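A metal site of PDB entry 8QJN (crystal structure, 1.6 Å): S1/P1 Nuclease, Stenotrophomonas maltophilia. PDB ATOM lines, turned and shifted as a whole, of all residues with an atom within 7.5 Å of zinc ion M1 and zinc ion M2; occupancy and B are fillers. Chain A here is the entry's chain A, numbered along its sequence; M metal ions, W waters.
The guanidinium group (NH1) of Arg 48 sits close to a ring nitrogen (ND1) of His 62 (3.2 Å).
O of His 62 sits at hydrogen-bond distance from ND1 of His 125, 2.7 Å away.
The backbone carbonyl oxygen (O) of His 115 sits close to a ring nitrogen (ND1) of His 6 (3.5 Å).
A ring nitrogen (ND1) of His 115 lies within hydrogen-bond range of the backbone carbonyl oxygen (O) of Ala 41 (2.8 Å).
The backbone NH of Trp 1 sits close to the side-chain carboxylate of Asp 153.
NE1 of Trp 1 sits at hydrogen-bond distance from O of Gly 118 (2.8 Å).
The side-chain carboxylate of Asp 45 sits close to the guanidinium group of Arg 48 (3.2 Å).
Residues that only touch zinc ion M1: Arg 48.
Five residues have an atom within 4 Å of zinc ion M1: Asp 45, Arg 48, His 62, His 115 and Asp 119.
Along chain A the residues within 4 Å of zinc ion M1 span positions 45 to 119.
The nearest printed residue that does not touch zinc ion M1 is His 6 (4.01 Å).
Five residues have an atom within 4 Å of zinc ion M2: Trp 1, His 6, Asp 45, His 115 and Asp 119.
Zinc ion M1 is bound by water W1 (1.8 Å).
Zinc ion M1 is bound by OD2 of Asp 119 (2.0 Å).
A ring nitrogen (ND1) of His 62 is bound to zinc ion M1 (2.0 Å).
NE2 of His 115 binds zinc ion M1, at 2.1 Å.
Zinc ion M1 is bound by OD1 of Asp 45.
NE2 of His 6 is bound to zinc ion M2.
Water W1 is bound to zinc ion M2 (2.0 Å).
OD1 of Asp 119 binds zinc ion M2 (2.1 Å).
N of Trp 1 binds zinc ion M2 (2.2 Å).
The backbone carbonyl oxygen (O) of Trp 1 binds zinc ion M2.
Water W2 binds zinc ion M2 (2.5 Å).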
ATOM      1  N   TRP A   1      15.301 -13.831   7.163  1.00  0.00           N
ATOM      2  CA  TRP A   1      15.514 -12.380   7.237  1.00  0.00           C
ATOM      3  C   TRP A   1      14.454 -11.743   8.138  1.00  0.00           C
ATOM      4  O   TRP A   1      13.356 -12.359   8.313  1.00  0.00           O
ATOM      5  CB  TRP A   1      15.473 -11.719   5.826  1.00  0.00           C
ATOM      6  CG  TRP A   1      16.427 -12.334   4.856  1.00  0.00           C
ATOM      7  CD1 TRP A   1      16.100 -13.212   3.854  1.00  0.00           C
ATOM      8  CD2 TRP A   1      17.850 -12.127   4.765  1.00  0.00           C
ATOM      9  NE1 TRP A   1      17.231 -13.589   3.178  1.00  0.00           N
ATOM     10  CE2 TRP A   1      18.317 -12.903   3.681  1.00  0.00           C
ATOM     11  CE3 TRP A   1      18.765 -11.305   5.442  1.00  0.00           C
ATOM     12  CZ2 TRP A   1      19.653 -12.910   3.291  1.00  0.00           C
ATOM     13  CZ3 TRP A   1      20.101 -11.350   5.086  1.00  0.00           C
ATOM     14  CH2 TRP A   1      20.552 -12.146   4.030  1.00  0.00           C
ATOM     15  N   GLY A   2      14.745 -10.545   8.611  1.00  0.00           N
ATOM     16  CA  GLY A   2      13.721  -9.614   9.123  1.00  0.00           C
ATOM     17  C   GLY A   2      12.922  -9.018   7.998  1.00  0.00           C
ATOM     18  O   GLY A   2      13.179  -9.381   6.823  1.00  0.00           O
ATOM     19  N   ALA A   3      11.993  -8.115   8.314  1.00  0.00           N
ATOM     20  CA  ALA A   3      10.998  -7.617   7.361  1.00  0.00           C
ATOM     21  C   ALA A   3      11.729  -6.955   6.186  1.00  0.00           C
ATOM     22  O   ALA A   3      11.357  -7.190   5.007  1.00  0.00           O
ATOM     23  CB  ALA A   3      10.024  -6.644   8.023  1.00  0.00           C
ATOM     24  N   GLY A   5      14.769  -7.309   4.904  1.00  0.00           N
ATOM     25  CA  GLY A   5      15.417  -8.274   4.001  1.00  0.00           C
ATOM     26  C   GLY A   5      14.386  -8.914   3.087  1.00  0.00           C
ATOM     27  O   GLY A   5      14.665  -9.030   1.861  1.00  0.00           O
ATOM     28  N   HIS A   6      13.245  -9.354   3.638  1.00  0.00           N
ATOM     29  CA  HIS A   6      12.170  -9.964   2.825  1.00  0.00           C
ATOM     30  C   HIS A   6      11.657  -8.987   1.789  1.00  0.00           C
ATOM     31  O   HIS A   6      11.512  -9.426   0.606  1.00  0.00           O
ATOM     32  CB  HIS A   6      11.048 -10.513   3.693  1.00  0.00           C
ATOM     33  CG  HIS A   6      11.510 -11.776   4.324  1.00  0.00           C
ATOM     34  ND1 HIS A   6      11.703 -12.923   3.593  1.00  0.00           N
ATOM     35  CD2 HIS A   6      11.861 -12.050   5.589  1.00  0.00           C
ATOM     36  CE1 HIS A   6      12.129 -13.874   4.409  1.00  0.00           C
ATOM     37  NE2 HIS A   6      12.252 -13.366   5.653  1.00  0.00           N
ATOM     38  N   ALA A  41       5.821  -9.664   1.377  1.00  0.00           N
ATOM     39  CA  ALA A  41       7.035 -10.490   1.563  1.00  0.00           C
ATOM     40  C   ALA A  41       7.205 -10.887   3.019  1.00  0.00           C
ATOM     41  O   ALA A  41       7.610 -12.023   3.280  1.00  0.00           O
ATOM     42  CB  ALA A  41       8.270  -9.821   1.028  1.00  0.00           C
ATOM     43  N   PRO A  42       6.938 -10.018   4.024  1.00  0.00           N
ATOM     44  CA  PRO A  42       7.065 -10.431   5.419  1.00  0.00           C
ATOM     45  C   PRO A  42       5.903 -11.230   6.021  1.00  0.00           C
ATOM     46  O   PRO A  42       6.025 -11.648   7.171  1.00  0.00           O
ATOM     47  CB  PRO A  42       7.179  -9.106   6.171  1.00  0.00           C
ATOM     48  CG  PRO A  42       7.444  -8.076   5.095  1.00  0.00           C
ATOM     49  CD  PRO A  42       6.675  -8.574   3.884  1.00  0.00           C
ATOM     50  N   ALA A  44       4.594 -14.199   5.932  1.00  0.00           N
ATOM     51  CA  ALA A  44       4.697 -15.553   6.526  1.00  0.00           C
ATOM     52  C   ALA A  44       5.202 -15.477   7.977  1.00  0.00           C
ATOM     53  O   ALA A  44       4.886 -16.385   8.775  1.00  0.00           O
ATOM     54  CB  ALA A  44       5.565 -16.431   5.664  1.00  0.00           C
ATOM     55  N   ASP A  45       5.977 -14.439   8.315  1.00  0.00           N
ATOM     56  CA  ASP A  45       6.520 -14.230   9.682  1.00  0.00           C
ATOM     57  C   ASP A  45       5.423 -13.704  10.614  1.00  0.00           C
ATOM     58  O   ASP A  45       5.517 -13.966  11.806  1.00  0.00           O
ATOM     59  CB  ASP A  45       7.735 -13.293   9.695  1.00  0.00           C
ATOM     60  CG  ASP A  45       9.042 -13.942   9.220  1.00  0.00           C
ATOM     61  OD1 ASP A  45       9.095 -15.179   9.090  1.00  0.00           O
ATOM     62  OD2 ASP A  45      10.023 -13.182   8.945  1.00  0.00           O
ATOM     63  N   GLN A  46       4.465 -12.940  10.102  1.00  0.00           N
ATOM     64  CA  GLN A  46       3.427 -12.273  10.923  1.00  0.00           C
ATOM     65  C   GLN A  46       2.336 -13.305  11.261  1.00  0.00           C
ATOM     66  O   GLN A  46       1.676 -13.162  12.268  1.00  0.00           O
ATOM     67  CB  GLN A  46       2.843 -11.063  10.202  1.00  0.00           C
ATOM     68  CG  GLN A  46       3.854 -10.077   9.629  1.00  0.00           C
ATOM     69  CD  GLN A  46       5.179  -9.949  10.336  1.00  0.00           C
ATOM     70  OE1 GLN A  46       5.258  -9.773  11.561  1.00  0.00           O
ATOM     71  NE2 GLN A  46       6.265  -9.990   9.566  1.00  0.00           N
ATOM     72  N   ARG A  48       2.955 -16.800  11.350  1.00  0.00           N
ATOM     73  CA  ARG A  48       3.670 -17.631  12.352  1.00  0.00           C
ATOM     74  C   ARG A  48       3.604 -16.964  13.730  1.00  0.00           C
ATOM     75  O   ARG A  48       3.513 -17.691  14.755  1.00  0.00           O
ATOM     76  CB  ARG A  48       5.127 -17.820  11.940  1.00  0.00           C
ATOM     77  CG  ARG A  48       5.917 -18.722  12.869  1.00  0.00           C
ATOM     78  CD  ARG A  48       7.408 -18.643  12.587  1.00  0.00           C
ATOM     79  NE  ARG A  48       7.899 -17.280  12.736  1.00  0.00           N
ATOM     80  CZ  ARG A  48       8.932 -16.760  12.069  1.00  0.00           C
ATOM     81  NH1 ARG A  48       9.599 -17.492  11.201  1.00  0.00           N
ATOM     82  NH2 ARG A  48       9.280 -15.500  12.273  1.00  0.00           N
ATOM     83  N   ALA A  59       5.465 -22.908  10.816  1.00  0.00           N
ATOM     84  CA  ALA A  59       6.605 -22.320  11.553  1.00  0.00           C
ATOM     85  C   ALA A  59       7.912 -23.014  11.134  1.00  0.00           C
ATOM     86  O   ALA A  59       8.912 -22.290  10.993  1.00  0.00           O
ATOM     87  CB  ALA A  59       6.385 -22.443  13.047  1.00  0.00           C
ATOM     88  N   TRP A  61       8.638 -24.218   8.302  1.00  0.00           N
ATOM     89  CA  TRP A  61       8.854 -24.074   6.849  1.00  0.00           C
ATOM     90  C   TRP A  61       9.933 -23.008   6.592  1.00  0.00           C
ATOM     91  O   TRP A  61      10.376 -22.899   5.459  1.00  0.00           O
ATOM     92  CB  TRP A  61       7.549 -23.669   6.167  1.00  0.00           C
ATOM     93  CG  TRP A  61       6.453 -24.683   6.206  1.00  0.00           C
ATOM     94  CD1 TRP A  61       6.424 -25.934   6.791  1.00  0.00           C
ATOM     95  CD2 TRP A  61       5.177 -24.492   5.580  1.00  0.00           C
ATOM     96  NE1 TRP A  61       5.189 -26.512   6.583  1.00  0.00           N
ATOM     97  CE2 TRP A  61       4.418 -25.654   5.860  1.00  0.00           C
ATOM     98  CE3 TRP A  61       4.615 -23.470   4.811  1.00  0.00           C
ATOM     99  CZ2 TRP A  61       3.142 -25.822   5.332  1.00  0.00           C
ATOM    100  CZ3 TRP A  61       3.329 -23.618   4.356  1.00  0.00           C
ATOM    101  CH2 TRP A  61       2.600 -24.769   4.648  1.00  0.00           C
ATOM    102  N   HIS A  62      10.306 -22.203   7.611  1.00  0.00           N
ATOM    103  CA  HIS A  62      11.225 -21.066   7.397  1.00  0.00           C
ATOM    104  C   HIS A  62      12.687 -21.528   7.352  1.00  0.00           C
ATOM    105  O   HIS A  62      13.548 -20.706   7.060  1.00  0.00           O
ATOM    106  CB  HIS A  62      10.990 -19.983   8.424  1.00  0.00           C
ATOM    107  CG  HIS A  62       9.657 -19.364   8.329  1.00  0.00           C
ATOM    108  ND1 HIS A  62       9.477 -18.011   8.096  1.00  0.00           N
ATOM    109  CD2 HIS A  62       8.432 -19.912   8.498  1.00  0.00           C
ATOM    110  CE1 HIS A  62       8.181 -17.776   8.060  1.00  0.00           C
ATOM    111  NE2 HIS A  62       7.513 -18.921   8.296  1.00  0.00           N
ATOM    112  N   TYR A  63      12.993 -22.760   7.688  1.00  0.00           N
ATOM    113  CA  TYR A  63      14.416 -23.166   7.822  1.00  0.00           C
ATOM    114  C   TYR A  63      14.604 -24.649   7.560  1.00  0.00           C
ATOM    115  O   TYR A  63      13.651 -25.411   7.352  1.00  0.00           O
ATOM    116  CB  TYR A  63      14.943 -22.768   9.205  1.00  0.00           C
ATOM    117  CG  TYR A  63      14.139 -23.306  10.335  1.00  0.00           C
ATOM    118  CD1 TYR A  63      14.382 -24.588  10.826  1.00  0.00           C
ATOM    119  CD2 TYR A  63      13.107 -22.573  10.900  1.00  0.00           C
ATOM    120  CE1 TYR A  63      13.620 -25.120  11.862  1.00  0.00           C
ATOM    121  CE2 TYR A  63      12.337 -23.092  11.926  1.00  0.00           C
ATOM    122  CZ  TYR A  63      12.595 -24.362  12.402  1.00  0.00           C
ATOM    123  OH  TYR A  63      11.845 -24.889  13.434  1.00  0.00           O
ATOM    124  N   ILE A  85      12.040 -25.840   4.914  1.00  0.00           N
ATOM    125  CA  ILE A  85      11.921 -24.843   3.811  1.00  0.00           C
ATOM    126  C   ILE A  85      12.119 -25.507   2.462  1.00  0.00           C
ATOM    127  O   ILE A  85      11.513 -24.990   1.485  1.00  0.00           O
ATOM    128  CB  ILE A  85      12.903 -23.679   4.024  1.00  0.00           C
ATOM    129  CG1 ILE A  85      12.574 -22.507   3.090  1.00  0.00           C
ATOM    130  CG2 ILE A  85      14.348 -24.140   3.890  1.00  0.00           C
ATOM    131  CD1 ILE A  85      13.210 -21.231   3.563  1.00  0.00           C
ATOM    132  N   HIS A 115       8.389 -15.252   0.406  1.00  0.00           N
ATOM    133  CA  HIS A 115       9.022 -15.237   1.738  1.00  0.00           C
ATOM    134  C   HIS A 115      10.113 -16.327   1.732  1.00  0.00           C
ATOM    135  O   HIS A 115      11.237 -16.041   2.172  1.00  0.00           O
ATOM    136  CB  HIS A 115       8.001 -15.500   2.853  1.00  0.00           C
ATOM    137  CG  HIS A 115       8.600 -15.309   4.208  1.00  0.00           C
ATOM    138  ND1 HIS A 115       8.595 -14.088   4.844  1.00  0.00           N
ATOM    139  CD2 HIS A 115       9.249 -16.158   5.032  1.00  0.00           C
ATOM    140  CE1 HIS A 115       9.184 -14.188   6.013  1.00  0.00           C
ATOM    141  NE2 HIS A 115       9.614 -15.437   6.164  1.00  0.00           N
ATOM    142  N   LEU A 116       9.747 -17.558   1.364  1.00  0.00           N
ATOM    143  CA  LEU A 116      10.690 -18.691   1.523  1.00  0.00           C
ATOM    144  C   LEU A 116      11.887 -18.551   0.573  1.00  0.00           C
ATOM    145  O   LEU A 116      12.950 -19.016   0.927  1.00  0.00           O
ATOM    146  CB  LEU A 116       9.944 -20.010   1.350  1.00  0.00           C
ATOM    147  CG  LEU A 116       8.853 -20.262   2.367  1.00  0.00           C
ATOM    148  CD1 LEU A 116       8.262 -21.625   2.108  1.00  0.00           C
ATOM    149  CD2 LEU A 116       9.349 -20.130   3.804  1.00  0.00           C
ATOM    150  N   GLY A 118      13.370 -15.805  -0.020  1.00  0.00           N
ATOM    151  CA  GLY A 118      14.191 -14.999   0.909  1.00  0.00           C
ATOM    152  C   GLY A 118      14.879 -15.899   1.946  1.00  0.00           C
ATOM    153  O   GLY A 118      16.119 -15.875   2.083  1.00  0.00           O
ATOM    154  N   ASP A 119      14.095 -16.629   2.738  1.00  0.00           N
ATOM    155  CA  ASP A 119      14.614 -17.317   3.940  1.00  0.00           C
ATOM    156  C   ASP A 119      15.620 -18.388   3.518  1.00  0.00           C
ATOM    157  O   ASP A 119      16.628 -18.591   4.253  1.00  0.00           O
ATOM    158  CB  ASP A 119      13.524 -17.899   4.824  1.00  0.00           C
ATOM    159  CG  ASP A 119      12.993 -16.967   5.877  1.00  0.00           C
ATOM    160  OD1 ASP A 119      13.581 -15.884   6.019  1.00  0.00           O
ATOM    161  OD2 ASP A 119      11.970 -17.347   6.590  1.00  0.00           O
ATOM    162  N   ILE A 120      15.408 -19.047   2.373  1.00  0.00           N
ATOM    163  CA  ILE A 120      16.331 -20.126   1.952  1.00  0.00           C
ATOM    164  C   ILE A 120      17.689 -19.563   1.501  1.00  0.00           C
ATOM    165  O   ILE A 120      18.617 -20.367   1.331  1.00  0.00           O
ATOM    166  CB  ILE A 120      15.656 -21.023   0.903  1.00  0.00           C
ATOM    167  CG1 ILE A 120      16.226 -22.435   0.902  1.00  0.00           C
ATOM    168  CG2 ILE A 120      15.719 -20.354  -0.461  1.00  0.00           C
ATOM    169  CD1 ILE A 120      15.386 -23.396   0.096  1.00  0.00           C
ATOM    170  N   GLN A 122      19.074 -17.050   3.468  1.00  0.00           N
ATOM    171  CA  GLN A 122      19.656 -16.543   4.744  1.00  0.00           C
ATOM    172  C   GLN A 122      20.478 -17.685   5.348  1.00  0.00           C
ATOM    173  O   GLN A 122      19.930 -18.703   5.758  1.00  0.00           O
ATOM    174  CB  GLN A 122      18.579 -16.062   5.717  1.00  0.00           C
ATOM    175  CG  GLN A 122      19.033 -14.922   6.642  1.00  0.00           C
ATOM    176  CD  GLN A 122      19.957 -15.331   7.758  1.00  0.00           C
ATOM    177  OE1 GLN A 122      21.049 -15.829   7.539  1.00  0.00           O
ATOM    178  NE2 GLN A 122      19.536 -15.070   8.995  1.00  0.00           N
ATOM    179  N   HIS A 125      19.379 -19.609   8.290  1.00  0.00           N
ATOM    180  CA  HIS A 125      18.149 -20.418   8.113  1.00  0.00           C
ATOM    181  C   HIS A 125      18.502 -21.814   7.554  1.00  0.00           C
ATOM    182  O   HIS A 125      17.568 -22.586   7.342  1.00  0.00           O
ATOM    183  CB  HIS A 125      17.142 -19.675   7.233  1.00  0.00           C
ATOM    184  CG  HIS A 125      16.368 -18.638   7.942  1.00  0.00           C
ATOM    185  ND1 HIS A 125      15.019 -18.706   8.053  1.00  0.00           N
ATOM    186  CD2 HIS A 125      16.743 -17.558   8.675  1.00  0.00           C
ATOM    187  CE1 HIS A 125      14.582 -17.713   8.797  1.00  0.00           C
ATOM    188  NE2 HIS A 125      15.603 -16.961   9.155  1.00  0.00           N
ATOM    189  N   HIS A 149      21.913 -15.406  14.826  1.00  0.00           N
ATOM    190  CA  HIS A 149      20.723 -15.473  13.956  1.00  0.00           C
ATOM    191  C   HIS A 149      20.196 -14.072  13.627  1.00  0.00           C
ATOM    192  O   HIS A 149      20.035 -13.767  12.385  1.00  0.00           O
ATOM    193  CB  HIS A 149      19.628 -16.353  14.529  1.00  0.00           C
ATOM    194  CG  HIS A 149      18.601 -16.618  13.494  1.00  0.00           C
ATOM    195  ND1 HIS A 149      18.610 -17.779  12.779  1.00  0.00           N
ATOM    196  CD2 HIS A 149      17.556 -15.892  13.038  1.00  0.00           C
ATOM    197  CE1 HIS A 149      17.623 -17.750  11.901  1.00  0.00           C
ATOM    198  NE2 HIS A 149      16.928 -16.630  12.055  1.00  0.00           N
ATOM    199  N   ASP A 153      19.834 -11.970  10.179  1.00  0.00           N
ATOM    200  CA  ASP A 153      18.467 -11.577   9.731  1.00  0.00           C
ATOM    201  C   ASP A 153      18.357 -10.056   9.547  1.00  0.00           C
ATOM    202  O   ASP A 153      17.724  -9.669   8.578  1.00  0.00           O
ATOM    203  CB  ASP A 153      17.364 -12.029  10.678  1.00  0.00           C
ATOM    204  CG  ASP A 153      16.819 -13.412  10.472  1.00  0.00           C
ATOM    205  OD1 ASP A 153      17.247 -14.095   9.534  1.00  0.00           O
ATOM    206  OD2 ASP A 153      15.930 -13.774  11.244  1.00  0.00           O
HETATM  207 ZN    ZN M   1      10.614 -16.393   7.719  1.00  0.00          ZN
HETATM  208 ZN    ZN M   2      13.176 -14.251   7.220  1.00  0.00          ZN
HETATM  209 ZN    ZN M   3      15.537 -15.758  10.853  1.00  0.00          ZN
HETATM  210  O   HOH W   1      11.947 -15.369   8.397  1.00  0.00           O
HETATM  211  O   HOH W   2      13.640 -14.556   9.649  1.00  0.00           O
